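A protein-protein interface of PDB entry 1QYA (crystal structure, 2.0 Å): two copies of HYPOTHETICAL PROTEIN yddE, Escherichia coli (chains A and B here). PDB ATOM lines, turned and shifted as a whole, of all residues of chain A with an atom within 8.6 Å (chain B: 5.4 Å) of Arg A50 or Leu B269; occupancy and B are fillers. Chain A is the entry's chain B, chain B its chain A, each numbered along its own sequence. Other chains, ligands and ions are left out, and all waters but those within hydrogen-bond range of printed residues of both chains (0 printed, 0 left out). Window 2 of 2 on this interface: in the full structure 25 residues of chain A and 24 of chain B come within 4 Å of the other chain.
NH2 of Arg B271 is in salt-bridge range of OE1 of Glu A51 (3.1 Å).
The backbone carbonyl oxygen (O) of Gly B270 is in hydrogen-bond range of the guanidinium group (NH2) of Arg A50.
The backbone carbonyl oxygen of Phe B26 lies within hydrogen-bond range of the guanidinium group of Arg A50, 2.8 Å away.
The backbone carbonyl oxygen (O) of Leu B269 lies within hydrogen-bond range of the guanidinium group (NH1) of Arg A50, at 3.0 Å.
The backbone NH (N) of Arg B271 is in hydrogen-bond range of the backbone carbonyl oxygen (O) of Gly B266, 2.9 Å away.
O of Arg B27 is in hydrogen-bond range of NH2 of Arg B271, 3.0 Å away.
The guanidinium group (NH1) of Arg B27 is in hydrogen-bond range of the backbone carbonyl oxygen (O) of Gly B270 (2.9 Å).
Arg B27 touches Leu A47 (NH2 to CD1, 3.9996 Å).
Ile A48 touches Phe B26.
Arg A50 touches Arg B27.
Arg B271 touches Arg A50.
OE1 of Glu A51 touches CA of Phe B26, at 3.5 Å.
Of the printed residues of chain B, Leu A47 touches Arg B27 (3.9996 Å).
Printed residues of chain B within 4 Å of Ile A48: Phe B26 (3.7 Å).
Arg A50 touches five residues of chain B.
Of the printed residues of chain B, Glu A51 touches Phe B26 and Arg B271.
Val A77 touches none of the printed residues of chain B.
Printed residues of chain A within 4 Å of Arg B27: Leu A47 (3.9996 Å) and Arg A50 (3.8 Å).
No residue of chain A comes within 4 Å of Ala B268.
Of the printed residues of chain A, Leu B269 touches Arg A50.
Gly B270 touches just one residue of chain A: Arg A50 (3.2 Å).
Of the printed residues of chain A, Arg B271 touches Arg A50 and Glu A51.
The nearest residue of chain A that does not touch Leu B269 is Leu A47 (7.6 Å).
The nearest printed residue of chain A that does not touch Arg B27 is Glu A51 (5.0 Å).
Printed residues of chain A that touch a printed residue of chain B: Leu A47, Ile A48, Arg A50 and Glu A51.
Hydrophobic or aromatic side chains of chain A within 4 Å of the printed part of chain B: Leu A47 and Ile A48.
Of the 11 printed residues of chain B, 5 touch a printed residue of chain A.
Hydrophobic or aromatic side chains of chain B that line the printed part of chain A: Phe B26.
Among the printed residues, 9 pairs touch across the chains.
Among the printed residues, Asp or Glu carboxylates within 4 Å of a Lys or Arg side-chain nitrogen of the other chain: Glu A51 with Arg B271.
No position is printed for both chains.
Of the 9 pairs that touch across the chains among the printed residues, none has its exchanged pair printed and touching as well.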
ATOM      1  N   ALA A  43     -26.662   7.904  10.052  1.00  0.00           N
ATOM      2  CA  ALA A  43     -27.431   7.206  11.081  1.00  0.00           C
ATOM      3  C   ALA A  43     -26.504   6.383  11.984  1.00  0.00           C
ATOM      4  O   ALA A  43     -26.652   6.407  13.206  1.00  0.00           O
ATOM      5  CB  ALA A  43     -28.530   6.320  10.454  1.00  0.00           C
ATOM      6  N   GLN A  44     -25.541   5.674  11.396  1.00  0.00           N
ATOM      7  CA  GLN A  44     -24.581   4.914  12.194  1.00  0.00           C
ATOM      8  C   GLN A  44     -23.720   5.830  13.080  1.00  0.00           C
ATOM      9  O   GLN A  44     -23.446   5.493  14.228  1.00  0.00           O
ATOM     10  CB  GLN A  44     -23.664   4.050  11.328  1.00  0.00           C
ATOM     11  CG  GLN A  44     -24.353   2.901  10.608  1.00  0.00           C
ATOM     12  CD  GLN A  44     -23.383   2.041   9.801  1.00  0.00           C
ATOM     13  OE1 GLN A  44     -22.750   2.513   8.830  1.00  0.00           O
ATOM     14  NE2 GLN A  44     -23.281   0.771  10.182  1.00  0.00           N
ATOM     15  N   MET A  45     -23.311   6.986  12.555  1.00  0.00           N
ATOM     16  CA  MET A  45     -22.475   7.900  13.332  1.00  0.00           C
ATOM     17  C   MET A  45     -23.247   8.438  14.540  1.00  0.00           C
ATOM     18  O   MET A  45     -22.687   8.556  15.621  1.00  0.00           O
ATOM     19  CB  MET A  45     -21.961   9.059  12.472  1.00  0.00           C
ATOM     20  CG  MET A  45     -20.971   8.630  11.384  1.00  0.00           C
ATOM     21  SD  MET A  45     -20.464  10.027  10.367  1.00  0.00           S
ATOM     22  CE  MET A  45     -19.460   9.256   9.193  1.00  0.00           C
ATOM     23  N   GLN A  46     -24.528   8.766  14.344  1.00  0.00           N
ATOM     24  CA  GLN A  46     -25.352   9.295  15.414  1.00  0.00           C
ATOM     25  C   GLN A  46     -25.573   8.224  16.500  1.00  0.00           C
ATOM     26  O   GLN A  46     -25.566   8.535  17.669  1.00  0.00           O
ATOM     27  CB  GLN A  46     -26.690   9.822  14.860  1.00  0.00           C
ATOM     28  CG  GLN A  46     -27.586  10.500  15.892  1.00  0.00           C
ATOM     29  CD  GLN A  46     -26.891  11.673  16.564  1.00  0.00           C
ATOM     30  OE1 GLN A  46     -26.853  12.774  16.013  1.00  0.00           O
ATOM     31  NE2 GLN A  46     -26.311  11.431  17.731  1.00  0.00           N
ATOM     32  N   LEU A  47     -25.777   6.971  16.096  1.00  0.00           N
ATOM     33  CA  LEU A  47     -25.961   5.863  17.042  1.00  0.00           C
ATOM     34  C   LEU A  47     -24.699   5.593  17.838  1.00  0.00           C
ATOM     35  O   LEU A  47     -24.778   5.306  19.028  1.00  0.00           O
ATOM     36  CB  LEU A  47     -26.371   4.557  16.319  1.00  0.00           C
ATOM     37  CG  LEU A  47     -27.856   4.355  16.037  1.00  0.00           C
ATOM     38  CD1 LEU A  47     -28.045   3.124  15.167  1.00  0.00           C
ATOM     39  CD2 LEU A  47     -28.660   4.234  17.322  1.00  0.00           C
ATOM     40  N   ILE A  48     -23.543   5.676  17.177  1.00  0.00           N
ATOM     41  CA  ILE A  48     -22.253   5.456  17.841  1.00  0.00           C
ATOM     42  C   ILE A  48     -21.980   6.559  18.847  1.00  0.00           C
ATOM     43  O   ILE A  48     -21.541   6.277  19.955  1.00  0.00           O
ATOM     44  CB  ILE A  48     -21.106   5.381  16.817  1.00  0.00           C
ATOM     45  CG1 ILE A  48     -21.201   4.076  16.029  1.00  0.00           C
ATOM     46  CG2 ILE A  48     -19.719   5.500  17.517  1.00  0.00           C
ATOM     47  CD1 ILE A  48     -20.370   4.057  14.763  1.00  0.00           C
ATOM     48  N   ALA A  49     -22.277   7.808  18.470  1.00  0.00           N
ATOM     49  CA  ALA A  49     -22.107   8.951  19.373  1.00  0.00           C
ATOM     50  C   ALA A  49     -23.019   8.801  20.602  1.00  0.00           C
ATOM     51  O   ALA A  49     -22.613   9.122  21.716  1.00  0.00           O
ATOM     52  CB  ALA A  49     -22.405  10.253  18.662  1.00  0.00           C
ATOM     53  N   ARG A  50     -24.251   8.343  20.388  1.00  0.00           N
ATOM     54  CA  ARG A  50     -25.163   8.079  21.509  1.00  0.00           C
ATOM     55  C   ARG A  50     -24.580   6.983  22.397  1.00  0.00           C
ATOM     56  O   ARG A  50     -24.524   7.127  23.609  1.00  0.00           O
ATOM     57  CB  ARG A  50     -26.550   7.670  21.016  1.00  0.00           C
ATOM     58  CG  ARG A  50     -27.599   7.690  22.143  1.00  0.00           C
ATOM     59  CD  ARG A  50     -28.936   7.136  21.765  1.00  0.00           C
ATOM     60  NE  ARG A  50     -28.848   5.747  21.301  1.00  0.00           N
ATOM     61  CZ  ARG A  50     -29.896   4.951  21.132  1.00  0.00           C
ATOM     62  NH1 ARG A  50     -31.119   5.390  21.394  1.00  0.00           N
ATOM     63  NH2 ARG A  50     -29.723   3.702  20.723  1.00  0.00           N
ATOM     64  N   GLU A  51     -24.077   5.925  21.763  1.00  0.00           N
ATOM     65  CA  GLU A  51     -23.538   4.756  22.466  1.00  0.00           C
ATOM     66  C   GLU A  51     -22.318   5.082  23.324  1.00  0.00           C
ATOM     67  O   GLU A  51     -22.208   4.587  24.441  1.00  0.00           O
ATOM     68  CB  GLU A  51     -23.157   3.642  21.472  1.00  0.00           C
ATOM     69  CG  GLU A  51     -22.914   2.286  22.130  1.00  0.00           C
ATOM     70  CD  GLU A  51     -24.134   1.743  22.824  1.00  0.00           C
ATOM     71  OE1 GLU A  51     -25.249   2.053  22.367  1.00  0.00           O
ATOM     72  OE2 GLU A  51     -23.993   1.009  23.829  1.00  0.00           O
ATOM     73  N   LEU A  52     -21.404   5.896  22.800  1.00  0.00           N
ATOM     74  CA  LEU A  52     -20.158   6.217  23.503  1.00  0.00           C
ATOM     75  C   LEU A  52     -20.400   7.206  24.653  1.00  0.00           C
ATOM     76  O   LEU A  52     -19.743   7.138  25.683  1.00  0.00           O
ATOM     77  CB  LEU A  52     -19.091   6.758  22.535  1.00  0.00           C
ATOM     78  CG  LEU A  52     -18.620   5.770  21.470  1.00  0.00           C
ATOM     79  CD1 LEU A  52     -17.583   6.410  20.596  1.00  0.00           C
ATOM     80  CD2 LEU A  52     -18.048   4.486  22.113  1.00  0.00           C
ATOM     81  N   GLY A  53     -21.344   8.119  24.478  1.00  0.00           N
ATOM     82  CA  GLY A  53     -21.786   8.958  25.584  1.00  0.00           C
ATOM     83  C   GLY A  53     -20.910  10.164  25.905  1.00  0.00           C
ATOM     84  O   GLY A  53     -21.200  10.860  26.876  1.00  0.00           O
ATOM     85  N   HIS A  54     -19.847  10.412  25.129  1.00  0.00           N
ATOM     86  CA  HIS A  54     -19.054  11.643  25.293  1.00  0.00           C
ATOM     87  C   HIS A  54     -19.909  12.847  24.890  1.00  0.00           C
ATOM     88  O   HIS A  54     -20.908  12.698  24.181  1.00  0.00           O
ATOM     89  CB  HIS A  54     -17.765  11.668  24.424  1.00  0.00           C
ATOM     90  CG  HIS A  54     -16.933  10.428  24.526  1.00  0.00           C
ATOM     91  ND1 HIS A  54     -16.307  10.039  25.688  1.00  0.00           N
ATOM     92  CD2 HIS A  54     -16.649   9.474  23.607  1.00  0.00           C
ATOM     93  CE1 HIS A  54     -15.683   8.892  25.484  1.00  0.00           C
ATOM     94  NE2 HIS A  54     -15.851   8.542  24.222  1.00  0.00           N
ATOM     95  N   SER A  55     -19.484  14.034  25.311  1.00  0.00           N
ATOM     96  CA  SER A  55     -20.133  15.268  24.884  1.00  0.00           C
ATOM     97  C   SER A  55     -20.066  15.362  23.360  1.00  0.00           C
ATOM     98  O   SER A  55     -21.029  15.782  22.735  1.00  0.00           O
ATOM     99  CB  SER A  55     -19.496  16.497  25.534  1.00  0.00           C
ATOM    100  OG  SER A  55     -18.167  16.683  25.070  1.00  0.00           O
ATOM    101  N   GLU A  56     -18.937  14.954  22.781  1.00  0.00           N
ATOM    102  CA  GLU A  56     -18.810  14.793  21.337  1.00  0.00           C
ATOM    103  C   GLU A  56     -17.985  13.570  20.957  1.00  0.00           C
ATOM    104  O   GLU A  56     -17.058  13.193  21.652  1.00  0.00           O
ATOM    105  CB  GLU A  56     -18.163  16.024  20.692  1.00  0.00           C
ATOM    106  CG  GLU A  56     -19.130  17.148  20.349  1.00  0.00           C
ATOM    107  CD  GLU A  56     -19.217  18.219  21.429  1.00  0.00           C
ATOM    108  OE1 GLU A  56     -18.477  18.130  22.437  1.00  0.00           O
ATOM    109  OE2 GLU A  56     -20.045  19.158  21.270  1.00  0.00           O
ATOM    110  N   THR A  57     -18.353  12.967  19.830  1.00  0.00           N
ATOM    111  CA  THR A  57     -17.536  11.998  19.128  1.00  0.00           C
ATOM    112  C   THR A  57     -17.251  12.553  17.731  1.00  0.00           C
ATOM    113  O   THR A  57     -18.155  13.071  17.057  1.00  0.00           O
ATOM    114  CB  THR A  57     -18.273  10.674  19.033  1.00  0.00           C
ATOM    115  OG1 THR A  57     -18.419  10.109  20.344  1.00  0.00           O
ATOM    116  CG2 THR A  57     -17.452   9.634  18.260  1.00  0.00           C
ATOM    117  N   PHE A  59     -15.636  11.927  13.826  1.00  0.00           N
ATOM    118  CA  PHE A  59     -15.536  10.861  12.828  1.00  0.00           C
ATOM    119  C   PHE A  59     -14.613  11.374  11.759  1.00  0.00           C
ATOM    120  O   PHE A  59     -14.867  12.430  11.196  1.00  0.00           O
ATOM    121  CB  PHE A  59     -16.916  10.543  12.263  1.00  0.00           C
ATOM    122  CG  PHE A  59     -17.818   9.891  13.264  1.00  0.00           C
ATOM    123  CD1 PHE A  59     -18.525  10.658  14.176  1.00  0.00           C
ATOM    124  CD2 PHE A  59     -17.920   8.511  13.333  1.00  0.00           C
ATOM    125  CE1 PHE A  59     -19.348  10.060  15.117  1.00  0.00           C
ATOM    126  CE2 PHE A  59     -18.721   7.909  14.293  1.00  0.00           C
ATOM    127  CZ  PHE A  59     -19.445   8.693  15.176  1.00  0.00           C
ATOM    128  N   PHE A  73     -20.603  14.690  16.335  1.00  0.00           N
ATOM    129  CA  PHE A  73     -21.929  14.386  16.846  1.00  0.00           C
ATOM    130  C   PHE A  73     -21.919  14.382  18.372  1.00  0.00           C
ATOM    131  O   PHE A  73     -21.008  13.820  18.977  1.00  0.00           O
ATOM    132  CB  PHE A  73     -22.374  13.007  16.368  1.00  0.00           C
ATOM    133  CG  PHE A  73     -22.651  12.913  14.884  1.00  0.00           C
ATOM    134  CD1 PHE A  73     -21.606  12.800  13.972  1.00  0.00           C
ATOM    135  CD2 PHE A  73     -23.953  12.917  14.411  1.00  0.00           C
ATOM    136  CE1 PHE A  73     -21.863  12.706  12.605  1.00  0.00           C
ATOM    137  CE2 PHE A  73     -24.223  12.824  13.057  1.00  0.00           C
ATOM    138  CZ  PHE A  73     -23.186  12.724  12.148  1.00  0.00           C
ATOM    139  N   THR A  74     -22.919  15.005  18.989  1.00  0.00           N
ATOM    140  CA  THR A  74     -23.216  14.765  20.402  1.00  0.00           C
ATOM    141  C   THR A  74     -24.060  13.487  20.489  1.00  0.00           C
ATOM    142  O   THR A  74     -24.344  12.868  19.451  1.00  0.00           O
ATOM    143  CB  THR A  74     -23.987  15.941  21.022  1.00  0.00           C
ATOM    144  OG1 THR A  74     -25.353  15.920  20.577  1.00  0.00           O
ATOM    145  CG2 THR A  74     -23.432  17.279  20.555  1.00  0.00           C
ATOM    146  N   PRO A  75     -24.456  13.059  21.695  1.00  0.00           N
ATOM    147  CA  PRO A  75     -25.377  11.919  21.816  1.00  0.00           C
ATOM    148  C   PRO A  75     -26.709  12.032  21.054  1.00  0.00           C
ATOM    149  O   PRO A  75     -27.315  10.984  20.799  1.00  0.00           O
ATOM    150  CB  PRO A  75     -25.608  11.808  23.334  1.00  0.00           C
ATOM    151  CG  PRO A  75     -24.340  12.351  23.926  1.00  0.00           C
ATOM    152  CD  PRO A  75     -24.001  13.524  23.018  1.00  0.00           C
ATOM    153  N   THR A  76     -27.142  13.249  20.698  1.00  0.00           N
ATOM    154  CA  THR A  76     -28.457  13.475  20.082  1.00  0.00           C
ATOM    155  C   THR A  76     -28.465  14.142  18.700  1.00  0.00           C
ATOM    156  O   THR A  76     -29.471  14.048  18.008  1.00  0.00           O
ATOM    157  CB  THR A  76     -29.348  14.348  21.011  1.00  0.00           C
ATOM    158  OG1 THR A  76     -28.667  15.556  21.355  1.00  0.00           O
ATOM    159  CG2 THR A  76     -29.579  13.673  22.362  1.00  0.00           C
ATOM    160  N   VAL A  77     -27.391  14.835  18.310  1.00  0.00           N
ATOM    161  CA  VAL A  77     -27.412  15.651  17.083  1.00  0.00           C
ATOM    162  C   VAL A  77     -26.012  15.944  16.515  1.00  0.00           C
ATOM    163  O   VAL A  77     -25.030  15.974  17.248  1.00  0.00           O
ATOM    164  CB  VAL A  77     -28.205  16.979  17.337  1.00  0.00           C
ATOM    165  CG1 VAL A  77     -27.370  17.991  18.130  1.00  0.00           C
ATOM    166  CG2 VAL A  77     -28.717  17.580  16.029  1.00  0.00           C
ATOM    167  N   PHE B  26     -26.245  -1.343  19.776  1.00  0.00           N
ATOM    168  CA  PHE B  26     -26.853  -0.026  19.997  1.00  0.00           C
ATOM    169  C   PHE B  26     -28.239  -0.059  20.630  1.00  0.00           C
ATOM    170  O   PHE B  26     -28.853   0.989  20.790  1.00  0.00           O
ATOM    171  CB  PHE B  26     -26.861   0.805  18.706  1.00  0.00           C
ATOM    172  CG  PHE B  26     -25.516   0.849  18.023  1.00  0.00           C
ATOM    173  CD1 PHE B  26     -24.388   1.280  18.716  1.00  0.00           C
ATOM    174  CD2 PHE B  26     -25.368   0.417  16.717  1.00  0.00           C
ATOM    175  CE1 PHE B  26     -23.157   1.312  18.115  1.00  0.00           C
ATOM    176  CE2 PHE B  26     -24.120   0.448  16.109  1.00  0.00           C
ATOM    177  CZ  PHE B  26     -23.012   0.906  16.820  1.00  0.00           C
ATOM    178  N   ARG B  27     -28.712  -1.240  21.023  1.00  0.00           N
ATOM    179  CA  ARG B  27     -30.004  -1.371  21.705  1.00  0.00           C
ATOM    180  C   ARG B  27     -29.726  -1.849  23.121  1.00  0.00           C
ATOM    181  O   ARG B  27     -28.617  -1.723  23.591  1.00  0.00           O
ATOM    182  CB  ARG B  27     -30.935  -2.335  20.954  1.00  0.00           C
ATOM    183  CG  ARG B  27     -31.218  -1.971  19.486  1.00  0.00           C
ATOM    184  CD  ARG B  27     -31.591  -0.513  19.242  1.00  0.00           C
ATOM    185  NE  ARG B  27     -31.439  -0.131  17.836  1.00  0.00           N
ATOM    186  CZ  ARG B  27     -31.646   1.083  17.348  1.00  0.00           C
ATOM    187  NH1 ARG B  27     -32.005   2.087  18.137  1.00  0.00           N
ATOM    188  NH2 ARG B  27     -31.496   1.301  16.041  1.00  0.00           N
ATOM    189  N   GLU B 231     -35.121   7.421  32.967  1.00  0.00           N
ATOM    190  CA  GLU B 231     -35.654   6.161  32.460  1.00  0.00           C
ATOM    191  C   GLU B 231     -34.546   5.162  32.183  1.00  0.00           C
ATOM    192  O   GLU B 231     -33.612   5.450  31.445  1.00  0.00           O
ATOM    193  CB  GLU B 231     -36.493   6.374  31.194  1.00  0.00           C
ATOM    194  CG  GLU B 231     -37.376   5.176  30.870  1.00  0.00           C
ATOM    195  CD  GLU B 231     -38.163   5.318  29.583  1.00  0.00           C
ATOM    196  OE1 GLU B 231     -38.191   6.421  29.015  1.00  0.00           O
ATOM    197  OE2 GLU B 231     -38.745   4.306  29.128  1.00  0.00           O
ATOM    198  N   ASP B 232     -34.671   3.989  32.788  1.00  0.00           N
ATOM    199  CA  ASP B 232     -33.744   2.877  32.576  1.00  0.00           C
ATOM    200  C   ASP B 232     -34.241   2.055  31.367  1.00  0.00           C
ATOM    201  O   ASP B 232     -35.423   1.722  31.294  1.00  0.00           O
ATOM    202  CB  ASP B 232     -33.695   2.025  33.846  1.00  0.00           C
ATOM    203  CG  ASP B 232     -32.607   0.957  33.801  1.00  0.00           C
ATOM    204  OD1 ASP B 232     -31.456   1.299  33.465  1.00  0.00           O
ATOM    205  OD2 ASP B 232     -32.817  -0.250  34.086  1.00  0.00           O
ATOM    206  N   PRO B 233     -33.376   1.787  30.388  1.00  0.00           N
ATOM    207  CA  PRO B 233     -33.777   1.028  29.199  1.00  0.00           C
ATOM    208  C   PRO B 233     -34.344  -0.372  29.462  1.00  0.00           C
ATOM    209  O   PRO B 233     -35.402  -0.667  28.956  1.00  0.00           O
ATOM    210  CB  PRO B 233     -32.482   0.947  28.382  1.00  0.00           C
ATOM    211  CG  PRO B 233     -31.669   2.100  28.836  1.00  0.00           C
ATOM    212  CD  PRO B 233     -31.997   2.290  30.278  1.00  0.00           C
ATOM    213  N   GLY B 266     -37.798  -0.566  26.778  1.00  0.00           N
ATOM    214  CA  GLY B 266     -36.825   0.325  26.181  1.00  0.00           C
ATOM    215  C   GLY B 266     -37.182   0.861  24.806  1.00  0.00           C
ATOM    216  O   GLY B 266     -36.388   1.595  24.233  1.00  0.00           O
ATOM    217  N   ARG B 267     -38.354   0.512  24.273  1.00  0.00           N
ATOM    218  CA  ARG B 267     -38.702   0.884  22.891  1.00  0.00           C
ATOM    219  C   ARG B 267     -38.743   2.404  22.653  1.00  0.00           C
ATOM    220  O   ARG B 267     -38.245   2.894  21.639  1.00  0.00           O
ATOM    221  CB  ARG B 267     -40.055   0.260  22.493  1.00  0.00           C
ATOM    222  CG  ARG B 267     -40.449   0.393  20.966  1.00  0.00           C
ATOM    223  CD  ARG B 267     -41.780  -0.298  20.600  1.00  0.00           C
ATOM    224  NE  ARG B 267     -42.774   0.011  21.633  1.00  0.00           N
ATOM    225  CZ  ARG B 267     -43.538  -0.855  22.291  1.00  0.00           C
ATOM    226  NH1 ARG B 267     -43.522  -2.147  22.016  1.00  0.00           N
ATOM    227  NH2 ARG B 267     -44.351  -0.419  23.243  1.00  0.00           N
ATOM    228  N   ALA B 268     -39.322   3.146  23.592  1.00  0.00           N
ATOM    229  CA  ALA B 268     -39.463   4.599  23.446  1.00  0.00           C
ATOM    230  C   ALA B 268     -38.120   5.309  23.479  1.00  0.00           C
ATOM    231  O   ALA B 268     -37.971   6.383  22.905  1.00  0.00           O
ATOM    232  CB  ALA B 268     -40.371   5.162  24.535  1.00  0.00           C
ATOM    233  N   LEU B 269     -37.129   4.699  24.131  1.00  0.00           N
ATOM    234  CA  LEU B 269     -35.771   5.250  24.157  1.00  0.00           C
ATOM    235  C   LEU B 269     -34.927   4.855  22.940  1.00  0.00           C
ATOM    236  O   LEU B 269     -33.786   5.298  22.811  1.00  0.00           O
ATOM    237  CB  LEU B 269     -35.047   4.801  25.429  1.00  0.00           C
ATOM    238  CG  LEU B 269     -35.609   5.313  26.751  1.00  0.00           C
ATOM    239  CD1 LEU B 269     -34.881   4.622  27.860  1.00  0.00           C
ATOM    240  CD2 LEU B 269     -35.450   6.824  26.857  1.00  0.00           C
ATOM    241  N   GLY B 270     -35.461   4.035  22.040  1.00  0.00           N
ATOM    242  CA  GLY B 270     -34.642   3.474  20.974  1.00  0.00           C
ATOM    243  C   GLY B 270     -33.610   2.477  21.530  1.00  0.00           C
ATOM    244  O   GLY B 270     -32.559   2.261  20.940  1.00  0.00           O
ATOM    245  N   ARG B 271     -33.925   1.865  22.667  1.00  0.00           N
ATOM    246  CA  ARG B 271     -33.017   0.950  23.361  1.00  0.00           C
ATOM    247  C   ARG B 271     -33.717  -0.367  23.753  1.00  0.00           C
ATOM    248  O   ARG B 271     -33.646  -0.836  24.893  1.00  0.00           O
ATOM    249  CB  ARG B 271     -32.422   1.663  24.574  1.00  0.00           C
ATOM    250  CG  ARG B 271     -31.505   2.852  24.175  1.00  0.00           C
ATOM    251  CD  ARG B 271     -30.324   3.039  25.107  1.00  0.00           C
ATOM    252  NE  ARG B 271     -29.387   1.936  24.938  1.00  0.00           N
ATOM    253  CZ  ARG B 271     -28.203   2.035  24.372  1.00  0.00           C
ATOM    254  NH1 ARG B 271     -27.737   3.212  23.979  1.00  0.00           N
ATOM    255  NH2 ARG B 271     -27.473   0.945  24.227  1.00  0.00           N
